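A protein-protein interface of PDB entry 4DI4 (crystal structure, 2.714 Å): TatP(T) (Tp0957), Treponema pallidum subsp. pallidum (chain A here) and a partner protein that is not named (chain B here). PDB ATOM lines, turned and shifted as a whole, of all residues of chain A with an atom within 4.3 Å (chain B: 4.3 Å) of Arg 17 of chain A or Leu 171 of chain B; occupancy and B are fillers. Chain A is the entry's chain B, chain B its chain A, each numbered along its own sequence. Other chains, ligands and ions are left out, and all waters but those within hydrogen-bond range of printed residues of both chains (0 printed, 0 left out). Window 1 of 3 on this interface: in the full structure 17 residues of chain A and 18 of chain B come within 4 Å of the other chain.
Among the printed residues, pairs that only touch across the chains: Pro 15 of chain A with Leu 171 of chain B (3.8 Å), Arg 17 of chain A with Phe 166 of chain B (3.5 Å), Arg 17 of chain A with Ala 167 of chain B (3.3 Å), Arg 17 of chain A with Pro 170 of chain B (3.9 Å), Ser 18 of chain A with Leu 171 of chain B (3.9 Å), Leu 200 of chain A with Leu 171 of chain B (3.95 Å) and Leu 200 of chain A with Gly 172 of chain B (3.96 Å).
O of Thr 169 of chain B is in hydrogen-bond range of NE of Arg 17 of chain A. N of Leu 171 of chain B sits close to O of Arg 17 of chain A (3.5 Å).
The backbone carbonyl oxygen of Pro 170 of chain B sits close to the side-chain hydroxyl of Ser 173 of chain B (3.4 Å).
Hydrophobic or aromatic side chains of chain A that line the printed part of chain B: Pro 15 and Leu 200. Among the printed residues, no Asp or Glu carboxylate lies within 4 Å of a Lys or Arg side-chain nitrogen of the other chain.
Of the printed residues of chain B, Arg 17 of chain A touches Phe 166, Ala 167, Thr 169, Pro 170 and Leu 171. Of the printed residues of chain A, Leu 171 of chain B touches Pro 15, Arg 17, Ser 18 and Leu 200. Printed residues of chain B within 4 Å of Ser 18 of chain A: Leu 171 (3.9 Å). Of the printed residues of chain B, Leu 200 of chain A touches Leu 171 and Gly 172. Printed residues of chain A within 4 Å of Pro 170 of chain B: Arg 17. Printed residues of chain A within 4 Å of Thr 169 of chain B: Arg 17 (2.9 Å). Printed residues of chain A within 4 Å of Ala 167 of chain B: Arg 17. Ala 16 of chain A touches none of the printed residues of chain B. The nearest printed residue of chain B that does not touch Arg 17 of chain A is Gly 172 of chain B (6.6 Å). The nearest printed residue of chain A that does not touch Thr 169 of chain B is Ser 18 of chain A (6.7 Å).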
ATOM      1  N   PRO A  15     -32.422  -1.285  22.314  1.00  0.00           N
ATOM      2  CA  PRO A  15     -31.163  -1.668  22.958  1.00  0.00           C
ATOM      3  C   PRO A  15     -30.113  -0.554  23.022  1.00  0.00           C
ATOM      4  O   PRO A  15     -30.087   0.342  22.178  1.00  0.00           O
ATOM      5  CB  PRO A  15     -30.664  -2.808  22.068  1.00  0.00           C
ATOM      6  CG  PRO A  15     -31.909  -3.401  21.503  1.00  0.00           C
ATOM      7  CD  PRO A  15     -32.819  -2.246  21.272  1.00  0.00           C
ATOM      8  N   ALA A  16     -29.233  -0.662  24.018  1.00  0.00           N
ATOM      9  CA  ALA A  16     -28.255   0.364  24.377  1.00  0.00           C
ATOM     10  C   ALA A  16     -27.470   0.981  23.225  1.00  0.00           C
ATOM     11  O   ALA A  16     -27.592   2.172  22.949  1.00  0.00           O
ATOM     12  CB  ALA A  16     -27.301  -0.183  25.412  1.00  0.00           C
ATOM     13  N   ARG A  17     -26.612   0.204  22.596  1.00  0.00           N
ATOM     14  CA  ARG A  17     -25.815   0.743  21.500  1.00  0.00           C
ATOM     15  C   ARG A  17     -26.335   0.439  20.112  1.00  0.00           C
ATOM     16  O   ARG A  17     -25.596   0.557  19.139  1.00  0.00           O
ATOM     17  CB  ARG A  17     -24.328   0.438  21.637  1.00  0.00           C
ATOM     18  CG  ARG A  17     -23.559   1.521  22.406  1.00  0.00           C
ATOM     19  CD  ARG A  17     -23.422   1.125  23.859  1.00  0.00           C
ATOM     20  NE  ARG A  17     -22.881  -0.223  23.925  1.00  0.00           N
ATOM     21  CZ  ARG A  17     -23.074  -1.061  24.931  1.00  0.00           C
ATOM     22  NH1 ARG A  17     -23.801  -0.671  25.974  1.00  0.00           N
ATOM     23  NH2 ARG A  17     -22.544  -2.284  24.881  1.00  0.00           N
ATOM     24  N   SER A  18     -27.569  -0.048  20.042  1.00  0.00           N
ATOM     25  CA  SER A  18     -28.167  -0.542  18.798  1.00  0.00           C
ATOM     26  C   SER A  18     -28.396   0.504  17.720  1.00  0.00           C
ATOM     27  O   SER A  18     -28.442   1.700  17.995  1.00  0.00           O
ATOM     28  CB  SER A  18     -29.500  -1.218  19.104  1.00  0.00           C
ATOM     29  OG  SER A  18     -30.290  -0.395  19.936  1.00  0.00           O
ATOM     30  N   ILE A  19     -28.538   0.025  16.488  1.00  0.00           N
ATOM     31  CA  ILE A  19     -28.914   0.862  15.354  1.00  0.00           C
ATOM     32  C   ILE A  19     -30.296   1.496  15.527  1.00  0.00           C
ATOM     33  O   ILE A  19     -30.543   2.614  15.063  1.00  0.00           O
ATOM     34  CB  ILE A  19     -28.883   0.068  14.032  1.00  0.00           C
ATOM     35  CG1 ILE A  19     -29.624  -1.258  14.176  1.00  0.00           C
ATOM     36  CG2 ILE A  19     -27.470  -0.214  13.626  1.00  0.00           C
ATOM     37  CD1 ILE A  19     -29.839  -1.959  12.849  1.00  0.00           C
ATOM     38  N   LEU A 200     -27.817 -11.156  16.081  1.00  0.00           N
ATOM     39  CA  LEU A 200     -27.098 -10.157  16.862  1.00  0.00           C
ATOM     40  C   LEU A 200     -27.037 -10.572  18.320  1.00  0.00           C
ATOM     41  O   LEU A 200     -26.041 -10.342  19.006  1.00  0.00           O
ATOM     42  CB  LEU A 200     -27.777  -8.804  16.734  1.00  0.00           C
ATOM     43  CG  LEU A 200     -27.070  -7.564  17.277  1.00  0.00           C
ATOM     44  CD1 LEU A 200     -25.812  -7.214  16.475  1.00  0.00           C
ATOM     45  CD2 LEU A 200     -28.032  -6.393  17.289  1.00  0.00           C
ATOM     46  N   PHE B 166     -15.977  -0.362  25.935  1.00  0.00           N
ATOM     47  CA  PHE B 166     -17.075  -1.233  25.623  1.00  0.00           C
ATOM     48  C   PHE B 166     -18.389  -0.432  25.713  1.00  0.00           C
ATOM     49  O   PHE B 166     -19.341  -0.653  24.964  1.00  0.00           O
ATOM     50  CB  PHE B 166     -17.037  -2.436  26.580  1.00  0.00           C
ATOM     51  CG  PHE B 166     -18.323  -3.230  26.614  1.00  0.00           C
ATOM     52  CD1 PHE B 166     -18.663  -4.090  25.563  1.00  0.00           C
ATOM     53  CD2 PHE B 166     -19.204  -3.109  27.701  1.00  0.00           C
ATOM     54  CE1 PHE B 166     -19.841  -4.825  25.611  1.00  0.00           C
ATOM     55  CE2 PHE B 166     -20.387  -3.835  27.753  1.00  0.00           C
ATOM     56  CZ  PHE B 166     -20.703  -4.703  26.709  1.00  0.00           C
ATOM     57  N   ALA B 167     -18.416   0.526  26.622  1.00  0.00           N
ATOM     58  CA  ALA B 167     -19.609   1.295  26.851  1.00  0.00           C
ATOM     59  C   ALA B 167     -19.901   2.252  25.677  1.00  0.00           C
ATOM     60  O   ALA B 167     -21.028   2.747  25.532  1.00  0.00           O
ATOM     61  CB  ALA B 167     -19.475   2.052  28.156  1.00  0.00           C
ATOM     62  N   THR B 169     -19.097   1.304  22.537  1.00  0.00           N
ATOM     63  CA  THR B 169     -18.941   0.414  21.403  1.00  0.00           C
ATOM     64  C   THR B 169     -20.292  -0.052  20.851  1.00  0.00           C
ATOM     65  O   THR B 169     -21.124  -0.572  21.597  1.00  0.00           O
ATOM     66  CB  THR B 169     -18.050  -0.779  21.817  1.00  0.00           C
ATOM     67  OG1 THR B 169     -16.732  -0.284  22.022  1.00  0.00           O
ATOM     68  CG2 THR B 169     -18.013  -1.852  20.754  1.00  0.00           C
ATOM     69  N   PRO B 170     -20.513   0.140  19.539  1.00  0.00           N
ATOM     70  CA  PRO B 170     -21.750  -0.278  18.856  1.00  0.00           C
ATOM     71  C   PRO B 170     -22.056  -1.734  19.135  1.00  0.00           C
ATOM     72  O   PRO B 170     -21.167  -2.578  19.058  1.00  0.00           O
ATOM     73  CB  PRO B 170     -21.412  -0.112  17.377  1.00  0.00           C
ATOM     74  CG  PRO B 170     -20.373   0.959  17.361  1.00  0.00           C
ATOM     75  CD  PRO B 170     -19.548   0.735  18.605  1.00  0.00           C
ATOM     76  N   LEU B 171     -23.306  -2.008  19.476  1.00  0.00           N
ATOM     77  CA  LEU B 171     -23.757  -3.344  19.815  1.00  0.00           C
ATOM     78  C   LEU B 171     -23.400  -4.290  18.687  1.00  0.00           C
ATOM     79  O   LEU B 171     -23.715  -4.032  17.526  1.00  0.00           O
ATOM     80  CB  LEU B 171     -25.259  -3.319  19.999  1.00  0.00           C
ATOM     81  CG  LEU B 171     -26.016  -4.552  20.462  1.00  0.00           C
ATOM     82  CD1 LEU B 171     -25.447  -5.029  21.781  1.00  0.00           C
ATOM     83  CD2 LEU B 171     -27.505  -4.186  20.588  1.00  0.00           C
ATOM     84  N   GLY B 172     -22.735  -5.389  19.031  1.00  0.00           N
ATOM     85  CA  GLY B 172     -22.275  -6.338  18.037  1.00  0.00           C
ATOM     86  C   GLY B 172     -20.825  -6.145  17.642  1.00  0.00           C
ATOM     87  O   GLY B 172     -20.222  -7.033  17.050  1.00  0.00           O
ATOM     88  N   SER B 173     -20.266  -4.981  17.955  1.00  0.00           N
ATOM     89  CA  SER B 173     -18.873  -4.701  17.626  1.00  0.00           C
ATOM     90  C   SER B 173     -17.885  -5.129  18.715  1.00  0.00           C
ATOM     91  O   SER B 173     -16.699  -5.247  18.445  1.00  0.00           O
ATOM     92  CB  SER B 173     -18.679  -3.228  17.292  1.00  0.00           C
ATOM     93  OG  SER B 173     -19.395  -2.889  16.125  1.00  0.00           O
